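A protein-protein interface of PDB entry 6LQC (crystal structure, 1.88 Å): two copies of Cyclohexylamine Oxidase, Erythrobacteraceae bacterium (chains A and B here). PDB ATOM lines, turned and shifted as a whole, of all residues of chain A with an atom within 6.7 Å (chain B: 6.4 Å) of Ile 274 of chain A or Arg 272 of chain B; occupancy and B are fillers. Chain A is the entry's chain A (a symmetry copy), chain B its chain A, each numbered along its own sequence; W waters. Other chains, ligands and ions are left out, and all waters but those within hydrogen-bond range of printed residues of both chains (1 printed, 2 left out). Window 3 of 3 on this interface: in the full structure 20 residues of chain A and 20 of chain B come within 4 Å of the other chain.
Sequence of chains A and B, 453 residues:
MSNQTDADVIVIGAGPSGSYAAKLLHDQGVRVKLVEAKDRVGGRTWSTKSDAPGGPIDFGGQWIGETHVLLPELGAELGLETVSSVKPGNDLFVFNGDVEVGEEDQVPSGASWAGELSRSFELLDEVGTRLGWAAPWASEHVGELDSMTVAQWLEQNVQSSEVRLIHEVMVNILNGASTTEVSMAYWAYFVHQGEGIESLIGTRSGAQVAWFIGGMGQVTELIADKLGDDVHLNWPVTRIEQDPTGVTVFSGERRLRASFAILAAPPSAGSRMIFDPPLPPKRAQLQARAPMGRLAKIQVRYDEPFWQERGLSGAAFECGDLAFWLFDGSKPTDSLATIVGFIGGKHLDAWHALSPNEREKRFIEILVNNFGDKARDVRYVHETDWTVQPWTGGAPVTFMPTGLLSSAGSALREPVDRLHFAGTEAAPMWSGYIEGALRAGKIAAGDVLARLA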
ATOM      1  N   VAL A 237     -26.668   3.862  17.865  1.00  0.00           N
ATOM      2  CA  VAL A 237     -27.186   4.448  19.123  1.00  0.00           C
ATOM      3  C   VAL A 237     -27.103   5.946  18.996  1.00  0.00           C
ATOM      4  O   VAL A 237     -25.996   6.484  18.680  1.00  0.00           O
ATOM      5  CB  VAL A 237     -26.436   3.920  20.349  1.00  0.00           C
ATOM      6  CG1 VAL A 237     -26.863   4.679  21.596  1.00  0.00           C
ATOM      7  CG2 VAL A 237     -26.684   2.433  20.496  1.00  0.00           C
ATOM      8  N   THR A 238     -28.216   6.612  19.245  1.00  0.00           N
ATOM      9  CA  THR A 238     -28.326   8.072  19.124  1.00  0.00           C
ATOM     10  C   THR A 238     -28.557   8.725  20.479  1.00  0.00           C
ATOM     11  O   THR A 238     -28.334   9.975  20.569  1.00  0.00           O
ATOM     12  CB  THR A 238     -29.412   8.436  18.108  1.00  0.00           C
ATOM     13  OG1 THR A 238     -30.617   7.787  18.520  1.00  0.00           O
ATOM     14  CG2 THR A 238     -29.032   7.984  16.716  1.00  0.00           C
ATOM     15  N   ARG A 239     -29.056   7.986  21.459  1.00  0.00           N
ATOM     16  CA  ARG A 239     -29.443   8.581  22.767  1.00  0.00           C
ATOM     17  C   ARG A 239     -29.348   7.506  23.849  1.00  0.00           C
ATOM     18  O   ARG A 239     -29.685   6.321  23.597  1.00  0.00           O
ATOM     19  CB  ARG A 239     -30.829   9.223  22.694  1.00  0.00           C
ATOM     20  CG  ARG A 239     -31.453   9.508  24.051  1.00  0.00           C
ATOM     21  CD  ARG A 239     -32.897   9.946  23.959  1.00  0.00           C
ATOM     22  NE  ARG A 239     -32.873  11.264  23.388  1.00  0.00           N
ATOM     23  CZ  ARG A 239     -32.985  12.391  24.059  1.00  0.00           C
ATOM     24  NH1 ARG A 239     -33.198  12.374  25.359  1.00  0.00           N
ATOM     25  NH2 ARG A 239     -32.893  13.529  23.398  1.00  0.00           N
ATOM     26  N   ILE A 240     -28.798   7.889  24.995  1.00  0.00           N
ATOM     27  CA  ILE A 240     -28.815   7.023  26.196  1.00  0.00           C
ATOM     28  C   ILE A 240     -29.509   7.804  27.285  1.00  0.00           C
ATOM     29  O   ILE A 240     -29.082   8.930  27.585  1.00  0.00           O
ATOM     30  CB  ILE A 240     -27.411   6.556  26.561  1.00  0.00           C
ATOM     31  CG1 ILE A 240     -26.827   5.709  25.424  1.00  0.00           C
ATOM     32  CG2 ILE A 240     -27.427   5.787  27.863  1.00  0.00           C
ATOM     33  CD1 ILE A 240     -25.367   5.284  25.622  1.00  0.00           C
ATOM     34  N   GLU A 241     -30.542   7.199  27.854  1.00  0.00           N
ATOM     35  CA  GLU A 241     -31.248   7.744  29.040  1.00  0.00           C
ATOM     36  C   GLU A 241     -31.025   6.800  30.197  1.00  0.00           C
ATOM     37  O   GLU A 241     -30.886   5.590  29.979  1.00  0.00           O
ATOM     38  CB  GLU A 241     -32.744   7.911  28.781  1.00  0.00           C
ATOM     39  CG  GLU A 241     -32.994   8.984  27.741  1.00  0.00           C
ATOM     40  CD  GLU A 241     -34.451   9.223  27.433  1.00  0.00           C
ATOM     41  OE1 GLU A 241     -35.308   8.500  27.990  1.00  0.00           O
ATOM     42  OE2 GLU A 241     -34.698  10.114  26.628  1.00  0.00           O
ATOM     43  N   GLY A 270     -19.078   8.134  21.476  1.00  0.00           N
ATOM     44  CA  GLY A 270     -19.917   8.638  22.562  1.00  0.00           C
ATOM     45  C   GLY A 270     -20.300  10.068  22.337  1.00  0.00           C
ATOM     46  O   GLY A 270     -21.484  10.450  22.611  1.00  0.00           O
ATOM     47  N   SER A 271     -19.400  10.873  21.756  1.00  0.00           N
ATOM     48  CA  SER A 271     -19.679  12.324  21.622  1.00  0.00           C
ATOM     49  C   SER A 271     -20.875  12.541  20.703  1.00  0.00           C
ATOM     50  O   SER A 271     -21.483  13.640  20.768  1.00  0.00           O
ATOM     51  CB  SER A 271     -18.476  13.119  21.127  1.00  0.00           C
ATOM     52  OG  SER A 271     -18.322  12.892  19.745  1.00  0.00           O
ATOM     53  N   ARG A 272     -21.226  11.592  19.833  1.00  0.00           N
ATOM     54  CA  ARG A 272     -22.339  11.857  18.874  1.00  0.00           C
ATOM     55  C   ARG A 272     -23.689  11.572  19.537  1.00  0.00           C
ATOM     56  O   ARG A 272     -24.701  11.873  18.921  1.00  0.00           O
ATOM     57  CB  ARG A 272     -22.265  11.017  17.596  1.00  0.00           C
ATOM     58  CG  ARG A 272     -20.906  10.386  17.371  1.00  0.00           C
ATOM     59  CD  ARG A 272     -19.879  11.194  16.611  1.00  0.00           C
ATOM     60  NE  ARG A 272     -20.006  11.017  15.171  1.00  0.00           N
ATOM     61  CZ  ARG A 272     -20.175   9.862  14.529  1.00  0.00           C
ATOM     62  NH1 ARG A 272     -20.215   8.720  15.191  1.00  0.00           N
ATOM     63  NH2 ARG A 272     -20.270   9.847  13.207  1.00  0.00           N
ATOM     64  N   MET A 273     -23.695  10.911  20.691  1.00  0.00           N
ATOM     65  CA  MET A 273     -24.943  10.499  21.377  1.00  0.00           C
ATOM     66  C   MET A 273     -25.416  11.610  22.305  1.00  0.00           C
ATOM     67  O   MET A 273     -24.615  12.413  22.764  1.00  0.00           O
ATOM     68  CB  MET A 273     -24.704   9.226  22.173  1.00  0.00           C
ATOM     69  CG  MET A 273     -24.127   8.107  21.355  1.00  0.00           C
ATOM     70  SD  MET A 273     -23.609   6.792  22.445  1.00  0.00           S
ATOM     71  CE  MET A 273     -22.851   5.696  21.255  1.00  0.00           C
ATOM     72  N   ILE A 274     -26.717  11.659  22.550  1.00  0.00           N
ATOM     73  CA  ILE A 274     -27.324  12.605  23.529  1.00  0.00           C
ATOM     74  C   ILE A 274     -27.566  11.811  24.792  1.00  0.00           C
ATOM     75  O   ILE A 274     -28.131  10.715  24.689  1.00  0.00           O
ATOM     76  CB  ILE A 274     -28.621  13.221  22.988  1.00  0.00           C
ATOM     77  CG1 ILE A 274     -28.361  13.956  21.682  1.00  0.00           C
ATOM     78  CG2 ILE A 274     -29.236  14.117  24.043  1.00  0.00           C
ATOM     79  CD1 ILE A 274     -27.438  15.131  21.826  1.00  0.00           C
ATOM     80  N   PHE A 275     -27.159  12.359  25.935  1.00  0.00           N
ATOM     81  CA  PHE A 275     -27.264  11.683  27.246  1.00  0.00           C
ATOM     82  C   PHE A 275     -28.267  12.457  28.094  1.00  0.00           C
ATOM     83  O   PHE A 275     -28.241  13.676  28.118  1.00  0.00           O
ATOM     84  CB  PHE A 275     -25.907  11.583  27.947  1.00  0.00           C
ATOM     85  CG  PHE A 275     -24.910  10.766  27.184  1.00  0.00           C
ATOM     86  CD1 PHE A 275     -24.197  11.325  26.129  1.00  0.00           C
ATOM     87  CD2 PHE A 275     -24.674   9.454  27.532  1.00  0.00           C
ATOM     88  CE1 PHE A 275     -23.291  10.554  25.417  1.00  0.00           C
ATOM     89  CE2 PHE A 275     -23.764   8.690  26.817  1.00  0.00           C
ATOM     90  CZ  PHE A 275     -23.099   9.242  25.750  1.00  0.00           C
ATOM     91  N   ASP A 276     -29.218  11.734  28.686  1.00  0.00           N
ATOM     92  CA  ASP A 276     -30.217  12.335  29.593  1.00  0.00           C
ATOM     93  C   ASP A 276     -30.370  11.403  30.772  1.00  0.00           C
ATOM     94  O   ASP A 276     -30.961  10.335  30.628  1.00  0.00           O
ATOM     95  CB  ASP A 276     -31.547  12.596  28.899  1.00  0.00           C
ATOM     96  CG  ASP A 276     -32.437  13.434  29.802  1.00  0.00           C
ATOM     97  OD1 ASP A 276     -32.002  13.748  30.919  1.00  0.00           O
ATOM     98  OD2 ASP A 276     -33.492  13.826  29.358  1.00  0.00           O
ATOM     99  N   PRO A 277     -29.836  11.749  31.960  1.00  0.00           N
ATOM    100  CA  PRO A 277     -29.227  13.052  32.200  1.00  0.00           C
ATOM    101  C   PRO A 277     -27.858  13.255  31.529  1.00  0.00           C
ATOM    102  O   PRO A 277     -27.185  12.308  31.140  1.00  0.00           O
ATOM    103  CB  PRO A 277     -29.061  13.086  33.724  1.00  0.00           C
ATOM    104  CG  PRO A 277     -29.025  11.651  34.152  1.00  0.00           C
ATOM    105  CD  PRO A 277     -29.883  10.909  33.158  1.00  0.00           C
ATOM    106  N   TRP A 391     -19.250   5.705  11.324  1.00  0.00           N
ATOM    107  CA  TRP A 391     -19.257   5.459  12.789  1.00  0.00           C
ATOM    108  C   TRP A 391     -17.867   5.010  13.279  1.00  0.00           C
ATOM    109  O   TRP A 391     -17.785   4.479  14.421  1.00  0.00           O
ATOM    110  CB  TRP A 391     -20.341   4.460  13.187  1.00  0.00           C
ATOM    111  CG  TRP A 391     -21.726   4.932  12.883  1.00  0.00           C
ATOM    112  CD1 TRP A 391     -22.457   5.880  13.547  1.00  0.00           C
ATOM    113  CD2 TRP A 391     -22.522   4.500  11.775  1.00  0.00           C
ATOM    114  NE1 TRP A 391     -23.655   6.073  12.917  1.00  0.00           N
ATOM    115  CE2 TRP A 391     -23.734   5.216  11.847  1.00  0.00           C
ATOM    116  CE3 TRP A 391     -22.340   3.537  10.771  1.00  0.00           C
ATOM    117  CZ2 TRP A 391     -24.776   5.002  10.939  1.00  0.00           C
ATOM    118  CZ3 TRP A 391     -23.365   3.341   9.864  1.00  0.00           C
ATOM    119  CH2 TRP A 391     -24.567   4.060   9.958  1.00  0.00           C
ATOM    120  N   VAL B 237     -30.753  16.246  12.796  1.00  0.00           N
ATOM    121  CA  VAL B 237     -30.226  15.663  11.541  1.00  0.00           C
ATOM    122  C   VAL B 237     -29.192  14.635  11.913  1.00  0.00           C
ATOM    123  O   VAL B 237     -28.237  14.964  12.685  1.00  0.00           O
ATOM    124  CB  VAL B 237     -29.673  16.740  10.602  1.00  0.00           C
ATOM    125  CG1 VAL B 237     -28.974  16.095   9.415  1.00  0.00           C
ATOM    126  CG2 VAL B 237     -30.797  17.651  10.153  1.00  0.00           C
ATOM    127  N   THR B 238     -29.350  13.436  11.385  1.00  0.00           N
ATOM    128  CA  THR B 238     -28.461  12.303  11.677  1.00  0.00           C
ATOM    129  C   THR B 238     -27.672  11.884  10.445  1.00  0.00           C
ATOM    130  O   THR B 238     -26.641  11.161  10.632  1.00  0.00           O
ATOM    131  CB  THR B 238     -29.265  11.145  12.277  1.00  0.00           C
ATOM    132  OG1 THR B 238     -30.323  10.842  11.366  1.00  0.00           O
ATOM    133  CG2 THR B 238     -29.835  11.517  13.626  1.00  0.00           C
ATOM    134  N   ARG B 239     -28.142  12.216   9.252  1.00  0.00           N
ATOM    135  CA  ARG B 239     -27.508  11.724   7.999  1.00  0.00           C
ATOM    136  C   ARG B 239     -27.795  12.719   6.874  1.00  0.00           C
ATOM    137  O   ARG B 239     -28.912  13.294   6.806  1.00  0.00           O
ATOM    138  CB  ARG B 239     -27.971  10.306   7.664  1.00  0.00           C
ATOM    139  CG  ARG B 239     -27.682   9.880   6.233  1.00  0.00           C
ATOM    140  CD  ARG B 239     -28.328   8.564   5.864  1.00  0.00           C
ATOM    141  NE  ARG B 239     -27.614   7.556   6.598  1.00  0.00           N
ATOM    142  CZ  ARG B 239     -26.671   6.779   6.110  1.00  0.00           C
ATOM    143  NH1 ARG B 239     -26.349   6.841   4.834  1.00  0.00           N
ATOM    144  NH2 ARG B 239     -26.069   5.932   6.924  1.00  0.00           N
ATOM    145  N   PRO B 267     -18.905  23.091  13.296  1.00  0.00           N
ATOM    146  CA  PRO B 267     -18.265  21.869  12.792  1.00  0.00           C
ATOM    147  C   PRO B 267     -18.487  20.667  13.713  1.00  0.00           C
ATOM    148  O   PRO B 267     -18.686  19.569  13.199  1.00  0.00           O
ATOM    149  CB  PRO B 267     -16.778  22.298  12.750  1.00  0.00           C
ATOM    150  CG  PRO B 267     -16.825  23.794  12.478  1.00  0.00           C
ATOM    151  CD  PRO B 267     -18.011  24.270  13.268  1.00  0.00           C
ATOM    152  N   SER B 268     -18.493  20.862  15.053  1.00  0.00           N
ATOM    153  CA  SER B 268     -18.714  19.766  16.028  1.00  0.00           C
ATOM    154  C   SER B 268     -20.112  19.136  15.807  1.00  0.00           C
ATOM    155  O   SER B 268     -20.242  17.934  16.005  1.00  0.00           O
ATOM    156  CB  SER B 268     -18.529  20.216  17.459  1.00  0.00           C
ATOM    157  OG  SER B 268     -19.261  21.425  17.730  1.00  0.00           O
ATOM    158  N   ALA B 269     -21.098  19.920  15.436  1.00  0.00           N
ATOM    159  CA  ALA B 269     -22.478  19.426  15.102  1.00  0.00           C
ATOM    160  C   ALA B 269     -22.443  18.539  13.868  1.00  0.00           C
ATOM    161  O   ALA B 269     -23.032  17.474  13.867  1.00  0.00           O
ATOM    162  CB  ALA B 269     -23.392  20.597  14.896  1.00  0.00           C
ATOM    163  N   GLY B 270     -21.723  18.957  12.850  1.00  0.00           N
ATOM    164  CA  GLY B 270     -21.517  18.187  11.624  1.00  0.00           C
ATOM    165  C   GLY B 270     -20.859  16.872  11.910  1.00  0.00           C
ATOM    166  O   GLY B 270     -21.248  15.830  11.289  1.00  0.00           O
ATOM    167  N   SER B 271     -19.947  16.828  12.890  1.00  0.00           N
ATOM    168  CA  SER B 271     -19.177  15.584  13.132  1.00  0.00           C
ATOM    169  C   SER B 271     -20.115  14.470  13.581  1.00  0.00           C
ATOM    170  O   SER B 271     -19.723  13.280  13.469  1.00  0.00           O
ATOM    171  CB  SER B 271     -18.049  15.769  14.142  1.00  0.00           C
ATOM    172  OG  SER B 271     -18.605  15.826  15.435  1.00  0.00           O
ATOM    173  N   ARG B 272     -21.301  14.774  14.112  1.00  0.00           N
ATOM    174  CA  ARG B 272     -22.168  13.676  14.634  1.00  0.00           C
ATOM    175  C   ARG B 272     -22.980  13.054  13.495  1.00  0.00           C
ATOM    176  O   ARG B 272     -23.635  12.052  13.744  1.00  0.00           O
ATOM    177  CB  ARG B 272     -23.158  14.132  15.711  1.00  0.00           C
ATOM    178  CG  ARG B 272     -22.812  15.479  16.312  1.00  0.00           C
ATOM    179  CD  ARG B 272     -21.882  15.493  17.503  1.00  0.00           C
ATOM    180  NE  ARG B 272     -22.602  15.315  18.756  1.00  0.00           N
ATOM    181  CZ  ARG B 272     -23.732  15.923  19.112  1.00  0.00           C
ATOM    182  NH1 ARG B 272     -24.303  16.810  18.316  1.00  0.00           N
ATOM    183  NH2 ARG B 272     -24.279  15.669  20.293  1.00  0.00           N
ATOM    184  N   MET B 273     -23.021  13.694  12.331  1.00  0.00           N
ATOM    185  CA  MET B 273     -23.846  13.236  11.188  1.00  0.00           C
ATOM    186  C   MET B 273     -23.050  12.261  10.330  1.00  0.00           C
ATOM    187  O   MET B 273     -21.827  12.307  10.319  1.00  0.00           O
ATOM    188  CB  MET B 273     -24.281  14.426  10.349  1.00  0.00           C
ATOM    189  CG  MET B 273     -24.979  15.494  11.140  1.00  0.00           C
ATOM    190  SD  MET B 273     -25.161  16.951  10.124  1.00  0.00           S
ATOM    191  CE  MET B 273     -25.861  18.071  11.327  1.00  0.00           C
ATOM    192  N   ILE B 274     -23.751  11.370   9.645  1.00  0.00           N
ATOM    193  CA  ILE B 274     -23.134  10.429   8.668  1.00  0.00           C
ATOM    194  C   ILE B 274     -23.376  11.019   7.298  1.00  0.00           C
ATOM    195  O   ILE B 274     -24.523  11.397   7.024  1.00  0.00           O
ATOM    196  CB  ILE B 274     -23.726   9.019   8.793  1.00  0.00           C
ATOM    197  CG1 ILE B 274     -23.528   8.476  10.200  1.00  0.00           C
ATOM    198  CG2 ILE B 274     -23.121   8.119   7.735  1.00  0.00           C
ATOM    199  CD1 ILE B 274     -22.086   8.295  10.577  1.00  0.00           C
ATOM    200  N   PHE B 275     -22.332  11.081   6.475  1.00  0.00           N
ATOM    201  CA  PHE B 275     -22.390  11.688   5.128  1.00  0.00           C
ATOM    202  C   PHE B 275     -22.188  10.578   4.103  1.00  0.00           C
ATOM    203  O   PHE B 275     -21.327   9.731   4.275  1.00  0.00           O
ATOM    204  CB  PHE B 275     -21.349  12.796   4.956  1.00  0.00           C
ATOM    205  CG  PHE B 275     -21.552  13.946   5.894  1.00  0.00           C
ATOM    206  CD1 PHE B 275     -21.097  13.878   7.206  1.00  0.00           C
ATOM    207  CD2 PHE B 275     -22.178  15.095   5.460  1.00  0.00           C
ATOM    208  CE1 PHE B 275     -21.310  14.940   8.071  1.00  0.00           C
ATOM    209  CE2 PHE B 275     -22.383  16.154   6.331  1.00  0.00           C
ATOM    210  CZ  PHE B 275     -21.968  16.056   7.635  1.00  0.00           C
ATOM    211  N   GLN B 287     -14.425  18.957  11.217  1.00  0.00           N
ATOM    212  CA  GLN B 287     -15.587  18.680  12.077  1.00  0.00           C
ATOM    213  C   GLN B 287     -15.168  17.875  13.321  1.00  0.00           C
ATOM    214  O   GLN B 287     -15.703  18.124  14.390  1.00  0.00           O
ATOM    215  CB  GLN B 287     -16.696  17.982  11.268  1.00  0.00           C
ATOM    216  CG  GLN B 287     -17.199  18.798  10.103  1.00  0.00           C
ATOM    217  CD  GLN B 287     -18.446  18.237   9.439  1.00  0.00           C
ATOM    218  OE1 GLN B 287     -19.251  18.995   8.922  1.00  0.00           O
ATOM    219  NE2 GLN B 287     -18.640  16.941   9.514  1.00  0.00           N
ATOM    220  N   PRO B 390     -28.132  20.160  24.952  1.00  0.00           N
ATOM    221  CA  PRO B 390     -28.086  19.064  23.987  1.00  0.00           C
ATOM    222  C   PRO B 390     -27.973  19.667  22.588  1.00  0.00           C
ATOM    223  O   PRO B 390     -28.576  20.676  22.336  1.00  0.00           O
ATOM    224  CB  PRO B 390     -29.389  18.254  24.213  1.00  0.00           C
ATOM    225  CG  PRO B 390     -30.301  19.312  24.811  1.00  0.00           C
ATOM    226  CD  PRO B 390     -29.402  20.168  25.695  1.00  0.00           C
ATOM    227  N   TRP B 391     -27.152  19.033  21.767  1.00  0.00           N
ATOM    228  CA  TRP B 391     -26.798  19.424  20.378  1.00  0.00           C
ATOM    229  C   TRP B 391     -26.050  20.772  20.360  1.00  0.00           C
ATOM    230  O   TRP B 391     -25.951  21.379  19.258  1.00  0.00           O
ATOM    231  CB  TRP B 391     -28.025  19.452  19.471  1.00  0.00           C
ATOM    232  CG  TRP B 391     -28.687  18.121  19.324  1.00  0.00           C
ATOM    233  CD1 TRP B 391     -28.260  17.045  18.593  1.00  0.00           C
ATOM    234  CD2 TRP B 391     -29.885  17.714  19.992  1.00  0.00           C
ATOM    235  NE1 TRP B 391     -29.112  15.991  18.770  1.00  0.00           N
ATOM    236  CE2 TRP B 391     -30.135  16.385  19.598  1.00  0.00           C
ATOM    237  CE3 TRP B 391     -30.792  18.373  20.836  1.00  0.00           C
ATOM    238  CZ2 TRP B 391     -31.267  15.685  20.026  1.00  0.00           C
ATOM    239  CZ3 TRP B 391     -31.901  17.673  21.273  1.00  0.00           C
ATOM    240  CH2 TRP B 391     -32.134  16.351  20.862  1.00  0.00           C
ATOM    241  N   THR B 392     -25.463  21.198  21.482  1.00  0.00           N
ATOM    242  CA  THR B 392     -24.507  22.341  21.466  1.00  0.00           C
ATOM    243  C   THR B 392     -23.266  21.915  22.250  1.00  0.00           C
ATOM    244  O   THR B 392     -22.210  21.781  21.634  1.00  0.00           O
ATOM    245  CB  THR B 392     -25.102  23.655  22.000  1.00  0.00           C
ATOM    246  OG1 THR B 392     -26.178  24.120  21.202  1.00  0.00           O
ATOM    247  CG2 THR B 392     -24.037  24.742  22.041  1.00  0.00           C
HETATM  248  O   HOH W   1     -18.154  14.489  17.659  1.00  0.00           O
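The backbone carbonyl oxygen of Ser 271 of chain B sits at hydrogen-bond distance from the guanidinium group of Arg 272 of chain A, at 2.8 Å.
NE of Arg 272 of chain B lies within hydrogen-bond range of O of Ser 271 of chain A (2.8 Å).
The backbone NH (N) of Ile 274 of chain B is in hydrogen-bond range of the backbone carbonyl oxygen (O) of Thr 238 of chain B, 3.1 Å away.
The backbone carbonyl oxygen of Ser 268 of chain B lies within hydrogen-bond range of the side-chain hydroxyl of Ser 271 of chain B.
The backbone carbonyl oxygen (O) of Thr 238 of chain A is in hydrogen-bond range of the backbone NH (N) of Ile 274 of chain A, 3.1 Å away.
NH1 of Arg 239 of chain A is in salt-bridge range of OE2 of Glu 241 of chain A (3.0 Å).
The backbone carbonyl oxygen of Ile 274 of chain A is in hydrogen-bond range of the backbone NH of Ile 240 of chain A (2.9 Å).
NH2 of Arg 239 of chain A touches CH2 of Trp 391 of chain B (3.9 Å).
Arg 272 of chain B touches Arg 272 of chain A (CA to NE, 3.5 Å).
NH2 of Arg 272 of chain A touches CD1 of Ile 274 of chain B, at 3.6 Å.
CD1 of Ile 274 of chain A touches NH2 of Arg 272 of chain B, at 3.6 Å.
Ile 274 of chain A touches Trp 391 of chain B.
Trp 391 of chain A touches Arg 239 of chain B (CH2 to NH2, 3.9 Å).
CD1 of Ile 274 of chain B touches NE1 of Trp 391 of chain A (3.6 Å).
Ile 240 of chain A touches none of the printed residues of chain B.
Of chain B, only Arg 272 and Trp 391 come within 4 Å of Ile 274 of chain A.
Arg 272 of chain B touches just these residues of chain A: Ser 271 (2.8 Å), Arg 272 (3.5 Å) and Ile 274 (3.6 Å).
Of the printed residues of chain A, Ile 274 of chain B touches Arg 272 and Trp 391.
Of the printed residues of chain A, Trp 391 of chain B touches Arg 239 and Ile 274.
The nearest printed residue of chain B that does not touch Arg 239 of chain A is Pro 390 of chain B (5.9 Å).
Printed residues of chain A that touch a printed residue of chain B: Arg 239, Ser 271, Arg 272, Ile 274 and Trp 391.
Hydrophobic or aromatic side chains of chain B that line the printed part of chain A: Ile 274 and Trp 391.
Along chain B the printed residues that touch a printed residue of chain A span positions 239 to 391.
Among the printed residues, no Asp or Glu carboxylate lies within 4 Å of a Lys or Arg side-chain nitrogen of the other chain.
Arg 239 of chain A touches Trp 391 of chain B, and with the chains exchanged Trp 391 of chain A touches Arg 239 of chain B.
Ser 271 of chain A touches Arg 272 of chain B, and with the chains exchanged Arg 272 of chain A touches Ser 271 of chain B.
Arg 272 of chain A touches its own counterpart, Arg 272 of chain B.
Ile 274 of chain A touches Trp 391 of chain B, and with the chains exchanged Trp 391 of chain A touches Ile 274 of chain B.
Water W1 bridges OG of Ser 271 of chain A and OG of Ser 271 of chain B.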
